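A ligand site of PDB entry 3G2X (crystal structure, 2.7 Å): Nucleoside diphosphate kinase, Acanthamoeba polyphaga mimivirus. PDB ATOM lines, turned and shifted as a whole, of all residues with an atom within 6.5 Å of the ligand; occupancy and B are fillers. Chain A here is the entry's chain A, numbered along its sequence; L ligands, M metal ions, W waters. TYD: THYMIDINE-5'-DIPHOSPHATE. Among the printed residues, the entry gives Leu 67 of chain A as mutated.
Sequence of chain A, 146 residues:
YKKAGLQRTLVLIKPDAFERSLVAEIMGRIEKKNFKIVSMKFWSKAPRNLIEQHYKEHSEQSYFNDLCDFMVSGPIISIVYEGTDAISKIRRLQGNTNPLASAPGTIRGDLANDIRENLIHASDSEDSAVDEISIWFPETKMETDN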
ATOM      1  N   LYS A  14      -1.355  19.730  30.037  1.00  0.00           N
ATOM      2  CA  LYS A  14      -0.806  20.074  28.728  1.00  0.00           C
ATOM      3  C   LYS A  14      -1.675  20.999  27.881  1.00  0.00           C
ATOM      4  O   LYS A  14      -2.881  21.073  28.056  1.00  0.00           O
ATOM      5  CB  LYS A  14      -0.477  18.794  27.954  1.00  0.00           C
ATOM      6  CG  LYS A  14       0.497  17.875  28.672  1.00  0.00           C
ATOM      7  CD  LYS A  14       0.851  16.682  27.795  1.00  0.00           C
ATOM      8  CE  LYS A  14       1.924  15.798  28.397  1.00  0.00           C
ATOM      9  NZ  LYS A  14       2.338  14.788  27.386  1.00  0.00           N
ATOM     10  N   TYR A  55      11.947  16.995  28.751  1.00  0.00           N
ATOM     11  CA  TYR A  55      11.937  15.775  27.947  1.00  0.00           C
ATOM     12  C   TYR A  55      13.330  15.301  27.453  1.00  0.00           C
ATOM     13  O   TYR A  55      13.409  14.557  26.463  1.00  0.00           O
ATOM     14  CB  TYR A  55      10.976  15.943  26.771  1.00  0.00           C
ATOM     15  CG  TYR A  55       9.542  15.843  27.180  1.00  0.00           C
ATOM     16  CD1 TYR A  55       8.675  16.910  27.049  1.00  0.00           C
ATOM     17  CD2 TYR A  55       9.062  14.676  27.757  1.00  0.00           C
ATOM     18  CE1 TYR A  55       7.358  16.819  27.453  1.00  0.00           C
ATOM     19  CE2 TYR A  55       7.749  14.569  28.167  1.00  0.00           C
ATOM     20  CZ  TYR A  55       6.903  15.637  28.010  1.00  0.00           C
ATOM     21  OH  TYR A  55       5.601  15.502  28.423  1.00  0.00           O
ATOM     22  N   HIS A  58      14.220  12.092  25.856  1.00  0.00           N
ATOM     23  CA  HIS A  58      13.498  11.815  24.608  1.00  0.00           C
ATOM     24  C   HIS A  58      14.163  12.455  23.388  1.00  0.00           C
ATOM     25  O   HIS A  58      13.732  12.251  22.255  1.00  0.00           O
ATOM     26  CB  HIS A  58      12.043  12.295  24.714  1.00  0.00           C
ATOM     27  CG  HIS A  58      11.209  11.487  25.657  1.00  0.00           C
ATOM     28  ND1 HIS A  58      10.479  10.393  25.242  1.00  0.00           N
ATOM     29  CD2 HIS A  58      11.020  11.585  26.993  1.00  0.00           C
ATOM     30  CE1 HIS A  58       9.871   9.857  26.285  1.00  0.00           C
ATOM     31  NE2 HIS A  58      10.177  10.563  27.355  1.00  0.00           N
ATOM     32  N   SER A  62      12.267  10.210  17.146  1.00  0.00           N
ATOM     33  CA  SER A  62      11.728  10.844  15.943  1.00  0.00           C
ATOM     34  C   SER A  62      10.791  11.977  16.306  1.00  0.00           C
ATOM     35  O   SER A  62      10.944  13.100  15.839  1.00  0.00           O
ATOM     36  CB  SER A  62      10.980   9.817  15.109  1.00  0.00           C
ATOM     37  OG  SER A  62      10.176   8.981  15.939  1.00  0.00           O
ATOM     38  N   TYR A  63       9.828  11.657  17.153  1.00  0.00           N
ATOM     39  CA  TYR A  63       8.746  12.563  17.551  1.00  0.00           C
ATOM     40  C   TYR A  63       9.168  13.718  18.489  1.00  0.00           C
ATOM     41  O   TYR A  63       8.363  14.582  18.791  1.00  0.00           O
ATOM     42  CB  TYR A  63       7.679  11.738  18.277  1.00  0.00           C
ATOM     43  CG  TYR A  63       8.179  11.114  19.566  1.00  0.00           C
ATOM     44  CD1 TYR A  63       8.415  11.893  20.688  1.00  0.00           C
ATOM     45  CD2 TYR A  63       8.424   9.746  19.664  1.00  0.00           C
ATOM     46  CE1 TYR A  63       8.871  11.346  21.867  1.00  0.00           C
ATOM     47  CE2 TYR A  63       8.879   9.179  20.856  1.00  0.00           C
ATOM     48  CZ  TYR A  63       9.103   9.989  21.950  1.00  0.00           C
ATOM     49  OH  TYR A  63       9.551   9.475  23.155  1.00  0.00           O
ATOM     50  N   PHE A  64      10.413  13.713  18.946  1.00  0.00           N
ATOM     51  CA  PHE A  64      10.843  14.701  19.937  1.00  0.00           C
ATOM     52  C   PHE A  64      10.598  16.142  19.536  1.00  0.00           C
ATOM     53  O   PHE A  64      10.466  17.033  20.385  1.00  0.00           O
ATOM     54  CB  PHE A  64      12.319  14.527  20.228  1.00  0.00           C
ATOM     55  CG  PHE A  64      12.842  15.486  21.243  1.00  0.00           C
ATOM     56  CD1 PHE A  64      13.592  16.570  20.862  1.00  0.00           C
ATOM     57  CD2 PHE A  64      12.604  15.285  22.590  1.00  0.00           C
ATOM     58  CE1 PHE A  64      14.101  17.449  21.799  1.00  0.00           C
ATOM     59  CE2 PHE A  64      13.108  16.160  23.534  1.00  0.00           C
ATOM     60  CZ  PHE A  64      13.861  17.240  23.141  1.00  0.00           C
ATOM     61  N   ASP A  66       8.036  17.264  17.346  1.00  0.00           N
ATOM     62  CA  ASP A  66       6.620  17.546  17.415  1.00  0.00           C
ATOM     63  C   ASP A  66       6.181  17.663  18.874  1.00  0.00           C
ATOM     64  O   ASP A  66       5.329  18.491  19.207  1.00  0.00           O
ATOM     65  CB  ASP A  66       5.847  16.477  16.670  1.00  0.00           C
ATOM     66  CG  ASP A  66       6.241  16.409  15.200  1.00  0.00           C
ATOM     67  OD1 ASP A  66       6.230  17.480  14.536  1.00  0.00           O
ATOM     68  OD2 ASP A  66       6.582  15.307  14.708  1.00  0.00           O
ATOM     69  N   LEU A  67       6.794  16.858  19.745  1.00  0.00           N
ATOM     70  CA  LEU A  67       6.525  16.947  21.171  1.00  0.00           C
ATOM     71  C   LEU A  67       6.802  18.332  21.746  1.00  0.00           C
ATOM     72  O   LEU A  67       5.896  18.974  22.289  1.00  0.00           O
ATOM     73  CB  LEU A  67       7.355  15.887  21.920  1.00  0.00           C
ATOM     74  CG  LEU A  67       7.292  15.850  23.456  1.00  0.00           C
ATOM     75  CD1 LEU A  67       5.860  15.763  23.938  1.00  0.00           C
ATOM     76  CD2 LEU A  67       8.117  14.712  24.009  1.00  0.00           C
ATOM     77  N   ARG A  91       0.294   7.906  38.259  1.00  0.00           N
ATOM     78  CA  ARG A  91       0.592   7.301  36.960  1.00  0.00           C
ATOM     79  C   ARG A  91      -0.507   6.314  36.522  1.00  0.00           C
ATOM     80  O   ARG A  91      -0.825   6.225  35.352  1.00  0.00           O
ATOM     81  CB  ARG A  91       1.955   6.603  36.976  1.00  0.00           C
ATOM     82  CG  ARG A  91       3.138   7.548  36.877  1.00  0.00           C
ATOM     83  CD  ARG A  91       3.367   8.037  35.455  1.00  0.00           C
ATOM     84  NE  ARG A  91       4.235   7.147  34.690  1.00  0.00           N
ATOM     85  CZ  ARG A  91       4.514   7.269  33.400  1.00  0.00           C
ATOM     86  NH1 ARG A  91       3.995   8.260  32.685  1.00  0.00           N
ATOM     87  NH2 ARG A  91       5.316   6.397  32.811  1.00  0.00           N
ATOM     88  N   GLN A  94      -3.420   8.535  35.262  1.00  0.00           N
ATOM     89  CA  GLN A  94      -3.027   9.080  33.976  1.00  0.00           C
ATOM     90  C   GLN A  94      -3.406   8.187  32.786  1.00  0.00           C
ATOM     91  O   GLN A  94      -3.971   8.654  31.795  1.00  0.00           O
ATOM     92  CB  GLN A  94      -1.523   9.343  33.988  1.00  0.00           C
ATOM     93  CG  GLN A  94      -0.944   9.835  32.663  1.00  0.00           C
ATOM     94  CD  GLN A  94       0.576   9.837  32.669  1.00  0.00           C
ATOM     95  OE1 GLN A  94       1.220  10.705  32.071  1.00  0.00           O
ATOM     96  NE2 GLN A  94       1.155   8.863  33.363  1.00  0.00           N
ATOM     97  N   GLY A  95      -3.099   6.893  32.883  1.00  0.00           N
ATOM     98  CA  GLY A  95      -3.352   5.979  31.791  1.00  0.00           C
ATOM     99  C   GLY A  95      -2.195   5.853  30.808  1.00  0.00           C
ATOM    100  O   GLY A  95      -1.224   6.628  30.840  1.00  0.00           O
ATOM    101  N   ASN A  96      -2.297   4.871  29.916  1.00  0.00           N
ATOM    102  CA  ASN A  96      -1.231   4.542  28.974  1.00  0.00           C
ATOM    103  C   ASN A  96      -1.041   5.635  27.926  1.00  0.00           C
ATOM    104  O   ASN A  96      -1.973   6.354  27.606  1.00  0.00           O
ATOM    105  CB  ASN A  96      -1.559   3.210  28.310  1.00  0.00           C
ATOM    106  CG  ASN A  96      -0.317   2.463  27.887  1.00  0.00           C
ATOM    107  OD1 ASN A  96       0.286   2.749  26.843  1.00  0.00           O
ATOM    108  ND2 ASN A  96       0.060   1.475  28.688  1.00  0.00           N
ATOM    109  N   THR A  97       0.161   5.765  27.377  1.00  0.00           N
ATOM    110  CA  THR A  97       0.434   6.820  26.406  1.00  0.00           C
ATOM    111  C   THR A  97      -0.312   6.606  25.103  1.00  0.00           C
ATOM    112  O   THR A  97      -0.733   7.556  24.446  1.00  0.00           O
ATOM    113  CB  THR A  97       1.923   6.934  26.112  1.00  0.00           C
ATOM    114  OG1 THR A  97       2.625   7.115  27.346  1.00  0.00           O
ATOM    115  CG2 THR A  97       2.197   8.122  25.214  1.00  0.00           C
ATOM    116  N   ARG A 108      -6.347   9.501  30.347  1.00  0.00           N
ATOM    117  CA  ARG A 108      -6.123   9.343  28.910  1.00  0.00           C
ATOM    118  C   ARG A 108      -7.139   8.380  28.264  1.00  0.00           C
ATOM    119  O   ARG A 108      -7.523   8.544  27.107  1.00  0.00           O
ATOM    120  CB  ARG A 108      -4.701   8.887  28.607  1.00  0.00           C
ATOM    121  CG  ARG A 108      -3.661   9.905  28.991  1.00  0.00           C
ATOM    122  CD  ARG A 108      -2.273   9.437  28.676  1.00  0.00           C
ATOM    123  NE  ARG A 108      -1.308  10.504  28.815  1.00  0.00           N
ATOM    124  CZ  ARG A 108      -0.018  10.315  29.043  1.00  0.00           C
ATOM    125  NH1 ARG A 108       0.448   9.091  29.180  1.00  0.00           N
ATOM    126  NH2 ARG A 108       0.796  11.341  29.151  1.00  0.00           N
ATOM    127  N   ILE A 115      -1.610   9.906  20.636  1.00  0.00           N
ATOM    128  CA  ILE A 115      -0.386   9.583  21.352  1.00  0.00           C
ATOM    129  C   ILE A 115       0.383  10.804  21.860  1.00  0.00           C
ATOM    130  O   ILE A 115       1.088  10.716  22.859  1.00  0.00           O
ATOM    131  CB  ILE A 115       0.532   8.720  20.478  1.00  0.00           C
ATOM    132  CG1 ILE A 115       1.414   7.817  21.344  1.00  0.00           C
ATOM    133  CG2 ILE A 115       1.346   9.601  19.538  1.00  0.00           C
ATOM    134  CD1 ILE A 115       1.861   6.584  20.637  1.00  0.00           C
ATOM    135  N   ARG A 116       0.265  11.936  21.182  1.00  0.00           N
ATOM    136  CA  ARG A 116       1.028  13.130  21.582  1.00  0.00           C
ATOM    137  C   ARG A 116       0.205  14.094  22.426  1.00  0.00           C
ATOM    138  O   ARG A 116       0.605  14.488  23.531  1.00  0.00           O
ATOM    139  CB  ARG A 116       1.612  13.854  20.362  1.00  0.00           C
ATOM    140  CG  ARG A 116       2.454  15.066  20.715  1.00  0.00           C
ATOM    141  CD  ARG A 116       2.704  15.948  19.496  1.00  0.00           C
ATOM    142  NE  ARG A 116       3.401  15.197  18.443  1.00  0.00           N
ATOM    143  CZ  ARG A 116       2.872  14.825  17.278  1.00  0.00           C
ATOM    144  NH1 ARG A 116       3.607  14.141  16.412  1.00  0.00           N
ATOM    145  NH2 ARG A 116       1.615  15.151  16.978  1.00  0.00           N
ATOM    146  N   GLU A 117      -0.938  14.503  21.892  1.00  0.00           N
ATOM    147  CA  GLU A 117      -1.864  15.347  22.611  1.00  0.00           C
ATOM    148  C   GLU A 117      -2.607  14.448  23.581  1.00  0.00           C
ATOM    149  O   GLU A 117      -3.690  13.976  23.270  1.00  0.00           O
ATOM    150  CB  GLU A 117      -2.812  16.019  21.618  1.00  0.00           C
ATOM    151  CG  GLU A 117      -2.111  16.477  20.356  1.00  0.00           C
ATOM    152  CD  GLU A 117      -2.878  17.517  19.566  1.00  0.00           C
ATOM    153  OE1 GLU A 117      -2.253  18.500  19.111  1.00  0.00           O
ATOM    154  OE2 GLU A 117      -4.095  17.352  19.387  1.00  0.00           O
ATOM    155  N   ASN A 118      -2.014  14.182  24.737  1.00  0.00           N
ATOM    156  CA  ASN A 118      -2.577  13.239  25.696  1.00  0.00           C
ATOM    157  C   ASN A 118      -2.820  13.861  27.047  1.00  0.00           C
ATOM    158  O   ASN A 118      -2.861  13.159  28.064  1.00  0.00           O
ATOM    159  CB  ASN A 118      -1.677  12.012  25.846  1.00  0.00           C
ATOM    160  CG  ASN A 118      -0.219  12.360  26.147  1.00  0.00           C
ATOM    161  OD1 ASN A 118       0.068  13.310  26.896  1.00  0.00           O
ATOM    162  ND2 ASN A 118       0.707  11.580  25.590  1.00  0.00           N
ATOM    163  N   ILE A 120      -1.890  15.084  29.837  1.00  0.00           N
ATOM    164  CA  ILE A 120      -1.258  15.155  31.150  1.00  0.00           C
ATOM    165  C   ILE A 120       0.068  14.434  31.246  1.00  0.00           C
ATOM    166  O   ILE A 120       0.170  13.282  30.835  1.00  0.00           O
ATOM    167  CB  ILE A 120      -2.177  14.576  32.261  1.00  0.00           C
ATOM    168  CG1 ILE A 120      -1.440  14.490  33.585  1.00  0.00           C
ATOM    169  CG2 ILE A 120      -2.673  13.198  31.897  1.00  0.00           C
ATOM    170  CD1 ILE A 120      -2.205  13.783  34.636  1.00  0.00           C
ATOM    171  N   HIS A 121       1.064  15.112  31.800  1.00  0.00           N
ATOM    172  CA  HIS A 121       2.304  14.454  32.175  1.00  0.00           C
ATOM    173  C   HIS A 121       2.312  14.148  33.667  1.00  0.00           C
ATOM    174  O   HIS A 121       1.769  14.891  34.470  1.00  0.00           O
ATOM    175  CB  HIS A 121       3.486  15.351  31.872  1.00  0.00           C
ATOM    176  CG  HIS A 121       4.762  14.847  32.467  1.00  0.00           C
ATOM    177  ND1 HIS A 121       5.589  13.959  31.821  1.00  0.00           N
ATOM    178  CD2 HIS A 121       5.337  15.079  33.670  1.00  0.00           C
ATOM    179  CE1 HIS A 121       6.622  13.676  32.578  1.00  0.00           C
ATOM    180  NE2 HIS A 121       6.501  14.358  33.713  1.00  0.00           N
ATOM    181  N   ALA A 122       2.933  13.033  34.027  1.00  0.00           N
ATOM    182  CA  ALA A 122       3.247  12.736  35.429  1.00  0.00           C
ATOM    183  C   ALA A 122       4.545  11.944  35.495  1.00  0.00           C
ATOM    184  O   ALA A 122       4.783  11.058  34.670  1.00  0.00           O
ATOM    185  CB  ALA A 122       2.125  11.980  36.098  1.00  0.00           C
ATOM    186  N   ASP A 124       7.512   9.439  36.044  1.00  0.00           N
ATOM    187  CA  ASP A 124       7.460   7.983  35.901  1.00  0.00           C
ATOM    188  C   ASP A 124       8.144   7.232  37.045  1.00  0.00           C
ATOM    189  O   ASP A 124       7.933   6.027  37.204  1.00  0.00           O
ATOM    190  CB  ASP A 124       7.965   7.499  34.531  1.00  0.00           C
ATOM    191  CG  ASP A 124       9.402   7.932  34.218  1.00  0.00           C
ATOM    192  OD1 ASP A 124      10.181   8.238  35.144  1.00  0.00           O
ATOM    193  OD2 ASP A 124       9.752   7.959  33.004  1.00  0.00           O
HETATM  194  PA  TYD L   1       6.445   8.787  27.328  1.00  0.00           P
HETATM  195  O1A TYD L   1       6.653   7.379  26.822  1.00  0.00           O
HETATM  196  O2A TYD L   1       7.274   9.378  28.452  1.00  0.00           O
HETATM  197  O3A TYD L   1       4.874   8.872  27.686  1.00  0.00           O
HETATM  198  PB  TYD L   1       4.278   9.411  29.085  1.00  0.00           P
HETATM  199  O1B TYD L   1       3.930  10.829  28.727  1.00  0.00           O
HETATM  200  O2B TYD L   1       5.313   9.276  30.154  1.00  0.00           O
HETATM  201  O3B TYD L   1       3.125   8.478  29.270  1.00  0.00           O
HETATM  202  O5' TYD L   1       6.497   9.777  26.081  1.00  0.00           O
HETATM  203  C5' TYD L   1       6.797  11.147  26.356  1.00  0.00           C
HETATM  204  C4' TYD L   1       5.870  12.052  25.554  1.00  0.00           C
HETATM  205  O4' TYD L   1       6.303  12.066  24.189  1.00  0.00           O
HETATM  206  C3' TYD L   1       4.433  11.545  25.534  1.00  0.00           C
HETATM  207  O3' TYD L   1       3.698  12.130  26.613  1.00  0.00           O
HETATM  208  C2' TYD L   1       3.914  11.924  24.164  1.00  0.00           C
HETATM  209  C1' TYD L   1       5.185  11.977  23.305  1.00  0.00           C
HETATM  210  N1  TYD L   1       5.265  10.771  22.457  1.00  0.00           N
HETATM  211  C2  TYD L   1       4.972  10.882  21.079  1.00  0.00           C
HETATM  212  O2  TYD L   1       4.675  12.011  20.617  1.00  0.00           O
HETATM  213  N3  TYD L   1       5.015   9.817  20.263  1.00  0.00           N
HETATM  214  C4  TYD L   1       5.340   8.612  20.724  1.00  0.00           C
HETATM  215  O4  TYD L   1       5.372   7.637  19.938  1.00  0.00           O
HETATM  216  C5  TYD L   1       5.657   8.468  22.186  1.00  0.00           C
HETATM  217  C5M TYD L   1       6.046   7.130  22.802  1.00  0.00           C
HETATM  218  C6  TYD L   1       5.612   9.601  22.989  1.00  0.00           C
HETATM  219 MG    MG M   1       7.521   9.734  31.602  1.00  0.00          MG
HETATM  220  O   HOH W   1       4.528  12.978  29.790  1.00  0.00           O
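NZ of Lys 14 is in hydrogen-bond range of O3' of the ligand, at 3.1 Å.
A ring nitrogen (NE2) of His 58 lies within hydrogen-bond range of an oxygen (O2A) of the ligand.
OG1 of Thr 97 is in hydrogen-bond range of O3B of the ligand (2.4 Å).
An oxygen (O3') of the ligand is in hydrogen-bond range of the side-chain amide nitrogen (ND2) of Asn 118, 3.2 Å away.
O2B of the ligand is in salt-bridge range of NH1 of Arg 91, 3.0 Å away.
NH1 of Arg 108 is in salt-bridge range of O3B of the ligand (2.7 Å).
The guanidinium group (NH2) of Arg 108 lies within hydrogen-bond range of the backbone carbonyl oxygen (O) of Ile 120, at 2.6 Å.
The side-chain hydroxyl (OH) of Tyr 63 lies within hydrogen-bond range of a ring nitrogen (ND1) of His 58.
NH1 of Arg 116 lies within salt-bridge range of OD2 of Asp 66, at 3.6 Å.
The side-chain hydroxyl (OH) of Tyr 55 is in hydrogen-bond range of the side-chain amino group (NZ) of Lys 14 (3.5 Å).
ND2 of Asn 118 lies within hydrogen-bond range of O of Ile 115.
O of Gln 94 sits at hydrogen-bond distance from N of Arg 108.
The side-chain amide nitrogen (NE2) of Gln 94 lies close to the guanidinium group (NH1) of Arg 91 (3.0 Å).
NH1 of Arg 108 is in hydrogen-bond range of OG1 of Thr 97, at 3.5 Å.
CE2 of Tyr 55 touches C5' of the ligand, 3.99 Å away.
Tyr 63 touches the ligand (CD2 to C4, 3.5 Å).
Leu 67 touches the ligand.
O of Ile 115 touches C2' of the ligand, 3.3 Å away.
Arg 116 touches the ligand (CB to O2, 3.6 Å).
Hydrophobic or aromatic side chains within 4 Å of the ligand: Tyr 55, His 58, Tyr 63, Leu 67 and Ile 115.
The nearest printed residue that does not touch the ligand is Gln 94 (4.1 Å).
Water W1 lies within hydrogen-bond range of O1B of the ligand (2.5 Å), ND1 of His 121 (2.5 Å) and OH of Tyr 55 (3.1 Å).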
